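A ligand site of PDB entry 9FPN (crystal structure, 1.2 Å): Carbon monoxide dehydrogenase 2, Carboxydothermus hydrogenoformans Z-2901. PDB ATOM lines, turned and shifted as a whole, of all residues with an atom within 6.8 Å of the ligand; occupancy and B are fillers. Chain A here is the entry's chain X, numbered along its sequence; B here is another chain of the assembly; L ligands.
SG of Cys 56 binds FE1 of the ligand, at 2.3 Å. The backbone NH (N) of Cys 51 lies close to a sulfur (S4) of the ligand, 3.7 Å away. A sulfur (S3) of the ligand sits close to the backbone NH of Cys 70, at 3.5 Å. SG of Cys 70 is bound to FE4 of the ligand, 2.4 Å away. A sulfur (S4) of the ligand sits close to the backbone NH (N) of His 50, 3.8 Å away. SG of Cys 51 binds FE2 of the ligand. SG of Cys 48 is bound to FE3 of the ligand (2.3 Å). A sulfur (S4) of the ligand lies close to the backbone NH (N) of Gly 54 (3.7 Å). The guanidinium group of Arg 80 lies close to a sulfur (S1) of the ligand (3.7 Å).
The backbone carbonyl oxygen (O) of Cys 56 lies close to the side-chain sulfur (SG) of Cys 47 (3.5 Å). The side-chain amide nitrogen (NE2) of Gln 38 of chain B sits at hydrogen-bond distance from the backbone carbonyl oxygen (O) of Gln 53 (2.9 Å). The side-chain sulfur of Cys 48 lies close to the guanidinium group of Arg 80, at 3.4 Å. SG of Cys 48 lies close to N of His 50, 3.4 Å away. N of Cys 48 sits at hydrogen-bond distance from O of Cys 56, 2.8 Å away. A ring nitrogen (ND1) of His 50 sits at hydrogen-bond distance from the backbone carbonyl oxygen (O) of Thr 197 (2.8 Å). The side-chain sulfur (SG) of Cys 51 lies close to the side-chain sulfur (SD) of Met 560 of chain B, 3.7 Å away. The side-chain sulfur (SG) of Cys 56 sits close to the backbone NH (N) of Ile 69 (3.5 Å).
NE2 of Gln 53 touches S3 of the ligand (3.8 Å). Gly 68 touches the ligand. Ile 69 touches the ligand (CB to S3, 3.8 Å). Met 199 touches the ligand. Hydrophobic or aromatic side chains that line the ligand: Ile 69 and Met 199. The nearest printed residue that does not touch the ligand is Ala 72 (4.02 Å).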
ATOM      1  N   CYS A  47     -13.714   0.668  14.589  1.00  0.00           N
ATOM      2  CA  CYS A  47     -13.013   0.003  15.673  1.00  0.00           C
ATOM      3  C   CYS A  47     -13.318  -1.479  15.576  1.00  0.00           C
ATOM      4  O   CYS A  47     -14.470  -1.866  15.296  1.00  0.00           O
ATOM      5  CB  CYS A  47     -13.387   0.506  17.058  1.00  0.00           C
ATOM      6  SG  CYS A  47     -12.552  -0.346  18.375  1.00  0.00           S
ATOM      7  N   CYS A  48     -12.312  -2.299  15.808  1.00  0.00           N
ATOM      8  CA  CYS A  48     -12.479  -3.748  15.842  1.00  0.00           C
ATOM      9  C   CYS A  48     -11.715  -4.337  17.018  1.00  0.00           C
ATOM     10  O   CYS A  48     -10.528  -4.018  17.218  1.00  0.00           O
ATOM     11  CB  CYS A  48     -11.982  -4.344  14.539  1.00  0.00           C
ATOM     12  SG  CYS A  48     -12.134  -6.169  14.465  1.00  0.00           S
ATOM     13  N   ARG A  49     -12.403  -5.215  17.763  1.00  0.00           N
ATOM     14  CA  ARG A  49     -11.841  -5.985  18.862  1.00  0.00           C
ATOM     15  C   ARG A  49     -12.108  -7.476  18.679  1.00  0.00           C
ATOM     16  O   ARG A  49     -12.250  -8.204  19.650  1.00  0.00           O
ATOM     17  CB  ARG A  49     -12.376  -5.464  20.188  1.00  0.00           C
ATOM     18  CG  ARG A  49     -12.057  -4.019  20.444  1.00  0.00           C
ATOM     19  CD  ARG A  49     -12.846  -3.528  21.636  1.00  0.00           C
ATOM     20  NE  ARG A  49     -12.603  -4.270  22.852  1.00  0.00           N
ATOM     21  CZ  ARG A  49     -13.411  -4.363  23.887  1.00  0.00           C
ATOM     22  NH1 ARG A  49     -14.543  -3.682  23.953  1.00  0.00           N
ATOM     23  NH2 ARG A  49     -13.056  -5.120  24.918  1.00  0.00           N
ATOM     24  N   HIS A  50     -12.130  -7.917  17.429  1.00  0.00           N
ATOM     25  CA  HIS A  50     -12.431  -9.317  17.130  1.00  0.00           C
ATOM     26  C   HIS A  50     -11.258 -10.256  17.355  1.00  0.00           C
ATOM     27  O   HIS A  50     -11.452 -11.474  17.202  1.00  0.00           O
ATOM     28  CB  HIS A  50     -13.062  -9.478  15.769  1.00  0.00           C
ATOM     29  CG  HIS A  50     -14.422  -8.842  15.620  1.00  0.00           C
ATOM     30  ND1 HIS A  50     -15.289  -9.177  14.611  1.00  0.00           N
ATOM     31  CD2 HIS A  50     -15.057  -7.898  16.343  1.00  0.00           C
ATOM     32  CE1 HIS A  50     -16.402  -8.443  14.714  1.00  0.00           C
ATOM     33  NE2 HIS A  50     -16.279  -7.646  15.759  1.00  0.00           N
ATOM     34  N   CYS A  51     -10.066  -9.773  17.702  1.00  0.00           N
ATOM     35  CA  CYS A  51      -9.012 -10.670  18.123  1.00  0.00           C
ATOM     36  C   CYS A  51      -8.085  -9.941  19.066  1.00  0.00           C
ATOM     37  O   CYS A  51      -8.193  -8.728  19.266  1.00  0.00           O
ATOM     38  CB  CYS A  51      -8.258 -11.283  16.933  1.00  0.00           C
ATOM     39  SG  CYS A  51      -6.983 -10.245  16.202  1.00  0.00           S
ATOM     40  N   LEU A  52      -7.193 -10.704  19.668  1.00  0.00           N
ATOM     41  CA  LEU A  52      -6.276 -10.183  20.664  1.00  0.00           C
ATOM     42  C   LEU A  52      -5.060  -9.479  20.072  1.00  0.00           C
ATOM     43  O   LEU A  52      -4.201  -9.040  20.861  1.00  0.00           O
ATOM     44  CB  LEU A  52      -5.846 -11.268  21.646  1.00  0.00           C
ATOM     45  CG  LEU A  52      -6.927 -12.011  22.379  1.00  0.00           C
ATOM     46  CD1 LEU A  52      -6.358 -12.982  23.368  1.00  0.00           C
ATOM     47  CD2 LEU A  52      -7.825 -11.004  23.089  1.00  0.00           C
ATOM     48  N   GLN A  53      -5.007  -9.317  18.746  1.00  0.00           N
ATOM     49  CA  GLN A  53      -4.088  -8.345  18.187  1.00  0.00           C
ATOM     50  C   GLN A  53      -4.600  -6.939  18.291  1.00  0.00           C
ATOM     51  O   GLN A  53      -3.820  -5.989  18.233  1.00  0.00           O
ATOM     52  CB  GLN A  53      -3.737  -8.654  16.739  1.00  0.00           C
ATOM     53  CG  GLN A  53      -2.918  -9.918  16.624  1.00  0.00           C
ATOM     54  CD  GLN A  53      -2.490 -10.336  15.239  1.00  0.00           C
ATOM     55  OE1 GLN A  53      -1.516 -11.059  15.098  1.00  0.00           O
ATOM     56  NE2 GLN A  53      -3.234  -9.943  14.219  1.00  0.00           N
ATOM     57  N   GLY A  54      -5.916  -6.773  18.471  1.00  0.00           N
ATOM     58  CA  GLY A  54      -6.501  -5.463  18.629  1.00  0.00           C
ATOM     59  C   GLY A  54      -6.299  -4.925  20.037  1.00  0.00           C
ATOM     60  O   GLY A  54      -5.587  -5.495  20.878  1.00  0.00           O
ATOM     61  N   PRO A  55      -6.963  -3.808  20.349  1.00  0.00           N
ATOM     62  CA  PRO A  55      -7.955  -3.165  19.503  1.00  0.00           C
ATOM     63  C   PRO A  55      -7.328  -2.489  18.281  1.00  0.00           C
ATOM     64  O   PRO A  55      -6.261  -1.843  18.356  1.00  0.00           O
ATOM     65  CB  PRO A  55      -8.580  -2.135  20.447  1.00  0.00           C
ATOM     66  CG  PRO A  55      -7.478  -1.852  21.440  1.00  0.00           C
ATOM     67  CD  PRO A  55      -6.781  -3.130  21.648  1.00  0.00           C
ATOM     68  N   CYS A  56      -8.041  -2.581  17.165  1.00  0.00           N
ATOM     69  CA  CYS A  56      -7.721  -1.874  15.931  1.00  0.00           C
ATOM     70  C   CYS A  56      -8.717  -0.759  15.696  1.00  0.00           C
ATOM     71  O   CYS A  56      -9.900  -0.858  16.082  1.00  0.00           O
ATOM     72  CB  CYS A  56      -7.749  -2.837  14.742  1.00  0.00           C
ATOM     73  SG  CYS A  56      -6.384  -4.021  14.770  1.00  0.00           S
ATOM     74  N   ARG A  57      -8.243   0.274  15.055  1.00  0.00           N
ATOM     75  CA  ARG A  57      -9.070   1.398  14.633  1.00  0.00           C
ATOM     76  C   ARG A  57      -8.565   1.917  13.311  1.00  0.00           C
ATOM     77  O   ARG A  57      -7.427   1.643  12.887  1.00  0.00           O
ATOM     78  CB  ARG A  57      -9.039   2.510  15.716  1.00  0.00           C
ATOM     79  CG  ARG A  57      -7.750   3.274  15.745  1.00  0.00           C
ATOM     80  CD  ARG A  57      -7.514   4.006  17.083  1.00  0.00           C
ATOM     81  NE  ARG A  57      -6.260   4.754  16.993  1.00  0.00           N
ATOM     82  CZ  ARG A  57      -5.068   4.181  17.047  1.00  0.00           C
ATOM     83  NH1 ARG A  57      -4.920   2.919  17.398  1.00  0.00           N
ATOM     84  NH2 ARG A  57      -3.996   4.909  16.705  1.00  0.00           N
ATOM     85  N   VAL A  67      -5.967   0.781   8.049  1.00  0.00           N
ATOM     86  CA  VAL A  67      -6.395  -0.605   7.856  1.00  0.00           C
ATOM     87  C   VAL A  67      -6.113  -1.359   9.136  1.00  0.00           C
ATOM     88  O   VAL A  67      -5.214  -1.013   9.896  1.00  0.00           O
ATOM     89  CB  VAL A  67      -5.591  -1.163   6.647  1.00  0.00           C
ATOM     90  CG1 VAL A  67      -4.117  -1.159   6.971  1.00  0.00           C
ATOM     91  CG2 VAL A  67      -6.110  -2.511   6.228  1.00  0.00           C
ATOM     92  N   GLY A  68      -6.910  -2.387   9.424  1.00  0.00           N
ATOM     93  CA  GLY A  68      -6.673  -3.188  10.588  1.00  0.00           C
ATOM     94  C   GLY A  68      -5.395  -4.005  10.491  1.00  0.00           C
ATOM     95  O   GLY A  68      -4.838  -4.198   9.404  1.00  0.00           O
ATOM     96  N   ILE A  69      -4.957  -4.524  11.640  1.00  0.00           N
ATOM     97  CA  ILE A  69      -3.679  -5.226  11.705  1.00  0.00           C
ATOM     98  C   ILE A  69      -3.654  -6.424  10.767  1.00  0.00           C
ATOM     99  O   ILE A  69      -2.651  -6.687  10.090  1.00  0.00           O
ATOM    100  CB  ILE A  69      -3.299  -5.592  13.155  1.00  0.00           C
ATOM    101  CG1 ILE A  69      -2.904  -4.290  13.878  1.00  0.00           C
ATOM    102  CG2 ILE A  69      -2.156  -6.601  13.204  1.00  0.00           C
ATOM    103  CD1 ILE A  69      -2.756  -4.414  15.346  1.00  0.00           C
ATOM    104  N   CYS A  70      -4.744  -7.203  10.707  1.00  0.00           N
ATOM    105  CA  CYS A  70      -4.816  -8.362   9.836  1.00  0.00           C
ATOM    106  C   CYS A  70      -5.044  -8.007   8.367  1.00  0.00           C
ATOM    107  O   CYS A  70      -5.093  -8.921   7.522  1.00  0.00           O
ATOM    108  CB  CYS A  70      -5.954  -9.271  10.284  1.00  0.00           C
ATOM    109  SG  CYS A  70      -7.574  -8.421  10.218  1.00  0.00           S
ATOM    110  N   GLY A  71      -5.236  -6.712   8.062  1.00  0.00           N
ATOM    111  CA  GLY A  71      -5.590  -6.265   6.740  1.00  0.00           C
ATOM    112  C   GLY A  71      -7.052  -5.883   6.570  1.00  0.00           C
ATOM    113  O   GLY A  71      -7.424  -5.463   5.471  1.00  0.00           O
ATOM    114  N   ALA A  72      -7.876  -6.025   7.597  1.00  0.00           N
ATOM    115  CA  ALA A  72      -9.307  -5.729   7.458  1.00  0.00           C
ATOM    116  C   ALA A  72      -9.517  -4.247   7.110  1.00  0.00           C
ATOM    117  O   ALA A  72      -8.998  -3.351   7.773  1.00  0.00           O
ATOM    118  CB  ALA A  72     -10.033  -6.053   8.753  1.00  0.00           C
ATOM    119  N   ILE A  77     -14.548  -4.012   8.544  1.00  0.00           N
ATOM    120  CA  ILE A  77     -14.756  -3.755   9.967  1.00  0.00           C
ATOM    121  C   ILE A  77     -16.177  -3.261  10.238  1.00  0.00           C
ATOM    122  O   ILE A  77     -16.854  -3.743  11.159  1.00  0.00           O
ATOM    123  CB  ILE A  77     -13.680  -2.783  10.487  1.00  0.00           C
ATOM    124  CG1 ILE A  77     -12.329  -3.528  10.532  1.00  0.00           C
ATOM    125  CG2 ILE A  77     -14.023  -2.160  11.827  1.00  0.00           C
ATOM    126  CD1 ILE A  77     -11.139  -2.590  10.821  1.00  0.00           C
ATOM    127  N   ARG A  80     -18.710  -6.090   9.622  1.00  0.00           N
ATOM    128  CA  ARG A  80     -18.666  -7.116  10.652  1.00  0.00           C
ATOM    129  C   ARG A  80     -19.324  -6.668  11.955  1.00  0.00           C
ATOM    130  O   ARG A  80     -20.052  -7.437  12.572  1.00  0.00           O
ATOM    131  CB  ARG A  80     -17.228  -7.559  10.919  1.00  0.00           C
ATOM    132  CG  ARG A  80     -16.613  -8.284   9.707  1.00  0.00           C
ATOM    133  CD  ARG A  80     -15.285  -9.003  10.035  1.00  0.00           C
ATOM    134  NE  ARG A  80     -14.331  -8.106  10.669  1.00  0.00           N
ATOM    135  CZ  ARG A  80     -13.025  -8.409  10.760  1.00  0.00           C
ATOM    136  NH1 ARG A  80     -12.565  -9.541  10.311  1.00  0.00           N
ATOM    137  NH2 ARG A  80     -12.183  -7.550  11.341  1.00  0.00           N
ATOM    138  N   THR A 197     -17.850 -13.359  10.905  1.00  0.00           N
ATOM    139  CA  THR A 197     -17.323 -12.067  11.337  1.00  0.00           C
ATOM    140  C   THR A 197     -16.101 -12.207  12.246  1.00  0.00           C
ATOM    141  O   THR A 197     -15.490 -11.174  12.612  1.00  0.00           O
ATOM    142  CB  THR A 197     -18.410 -11.226  12.045  1.00  0.00           C
ATOM    143  OG1 THR A 197     -18.882 -11.938  13.180  1.00  0.00           O
ATOM    144  CG2 THR A 197     -19.524 -10.882  11.084  1.00  0.00           C
ATOM    145  N   SER A 198     -15.754 -13.425  12.640  1.00  0.00           N
ATOM    146  CA  SER A 198     -14.559 -13.637  13.444  1.00  0.00           C
ATOM    147  C   SER A 198     -13.326 -13.473  12.575  1.00  0.00           C
ATOM    148  O   SER A 198     -13.392 -13.339  11.363  1.00  0.00           O
ATOM    149  CB  SER A 198     -14.550 -15.023  14.116  1.00  0.00           C
ATOM    150  OG  SER A 198     -14.329 -16.127  13.227  1.00  0.00           O
ATOM    151  N   MET A 199     -12.168 -13.383  13.225  1.00  0.00           N
ATOM    152  CA  MET A 199     -10.981 -12.961  12.495  1.00  0.00           C
ATOM    153  C   MET A 199     -10.636 -13.925  11.374  1.00  0.00           C
ATOM    154  O   MET A 199     -10.672 -15.168  11.537  1.00  0.00           O
ATOM    155  CB  MET A 199      -9.797 -12.797  13.451  1.00  0.00           C
ATOM    156  CG  MET A 199      -8.468 -12.370  12.784  1.00  0.00           C
ATOM    157  SD  MET A 199      -7.545 -13.808  12.114  1.00  0.00           S
ATOM    158  CE  MET A 199      -6.648 -13.086  10.735  1.00  0.00           C
ATOM    159  N   GLY A 200     -10.244 -13.353  10.237  1.00  0.00           N
ATOM    160  CA  GLY A 200      -9.739 -14.174   9.157  1.00  0.00           C
ATOM    161  C   GLY A 200     -10.768 -14.993   8.419  1.00  0.00           C
ATOM    162  O   GLY A 200     -10.428 -16.021   7.818  1.00  0.00           O
ATOM    163  N   MET B  35      -0.635   1.053  14.013  1.00  0.00           N
ATOM    164  CA  MET B  35      -1.745   1.077  14.943  1.00  0.00           C
ATOM    165  C   MET B  35      -1.350   1.579  16.321  1.00  0.00           C
ATOM    166  O   MET B  35      -2.213   1.834  17.145  1.00  0.00           O
ATOM    167  CB  MET B  35      -2.316  -0.342  15.048  1.00  0.00           C
ATOM    168  CG  MET B  35      -3.735  -0.369  15.618  1.00  0.00           C
ATOM    169  SD  MET B  35      -4.935   0.446  14.549  1.00  0.00           S
ATOM    170  CE  MET B  35      -4.974  -0.495  13.127  1.00  0.00           C
ATOM    171  N   GLN B  38      -2.132   1.596  20.747  1.00  0.00           N
ATOM    172  CA  GLN B  38      -3.475   1.071  20.654  1.00  0.00           C
ATOM    173  C   GLN B  38      -4.317   1.615  21.809  1.00  0.00           C
ATOM    174  O   GLN B  38      -3.808   2.045  22.836  1.00  0.00           O
ATOM    175  CB  GLN B  38      -3.464  -0.465  20.665  1.00  0.00           C
ATOM    176  CG  GLN B  38      -2.828  -1.005  19.419  1.00  0.00           C
ATOM    177  CD  GLN B  38      -2.718  -2.485  19.370  1.00  0.00           C
ATOM    178  OE1 GLN B  38      -1.795  -3.052  19.968  1.00  0.00           O
ATOM    179  NE2 GLN B  38      -3.653  -3.135  18.690  1.00  0.00           N
ATOM    180  N   PRO B 336      -6.846 -10.943   5.601  1.00  0.00           N
ATOM    181  CA  PRO B 336      -7.402 -10.514   4.305  1.00  0.00           C
ATOM    182  C   PRO B 336      -6.425  -9.713   3.478  1.00  0.00           C
ATOM    183  O   PRO B 336      -6.635  -9.584   2.282  1.00  0.00           O
ATOM    184  CB  PRO B 336      -8.660  -9.738   4.704  1.00  0.00           C
ATOM    185  CG  PRO B 336      -8.396  -9.300   6.105  1.00  0.00           C
ATOM    186  CD  PRO B 336      -7.629 -10.397   6.737  1.00  0.00           C
ATOM    187  N   MET B 560      -4.359 -15.292  19.939  1.00  0.00           N
ATOM    188  CA  MET B 560      -4.894 -14.255  19.075  1.00  0.00           C
ATOM    189  C   MET B 560      -6.413 -14.394  18.858  1.00  0.00           C
ATOM    190  O   MET B 560      -7.175 -13.452  19.097  1.00  0.00           O
ATOM    191  CB  MET B 560      -4.147 -14.224  17.727  1.00  0.00           C
ATOM    192  CG  MET B 560      -4.605 -13.161  16.770  1.00  0.00           C
ATOM    193  SD  MET B 560      -5.889 -13.711  15.572  1.00  0.00           S
ATOM    194  CE  MET B 560      -5.081 -15.046  14.729  1.00  0.00           C
HETATM  195 FE1  LIG L   1      -7.516  -6.021  14.360  1.00  0.00          FE
HETATM  196 FE2  LIG L   1      -8.028  -8.564  15.044  1.00  0.00          FE
HETATM  197 FE3  LIG L   1      -9.963  -6.919  14.198  1.00  0.00          FE
HETATM  198 FE4  LIG L   1      -8.158  -7.766  12.401  1.00  0.00          FE
HETATM  199  S1  LIG L   1      -9.676  -9.021  13.549  1.00  0.00           S
HETATM  200  S2  LIG L   1      -8.935  -5.702  12.599  1.00  0.00           S
HETATM  201  S3  LIG L   1      -6.316  -7.754  13.732  1.00  0.00           S
HETATM  202  S4  LIG L   1      -8.783  -6.768  16.074  1.00  0.00           S
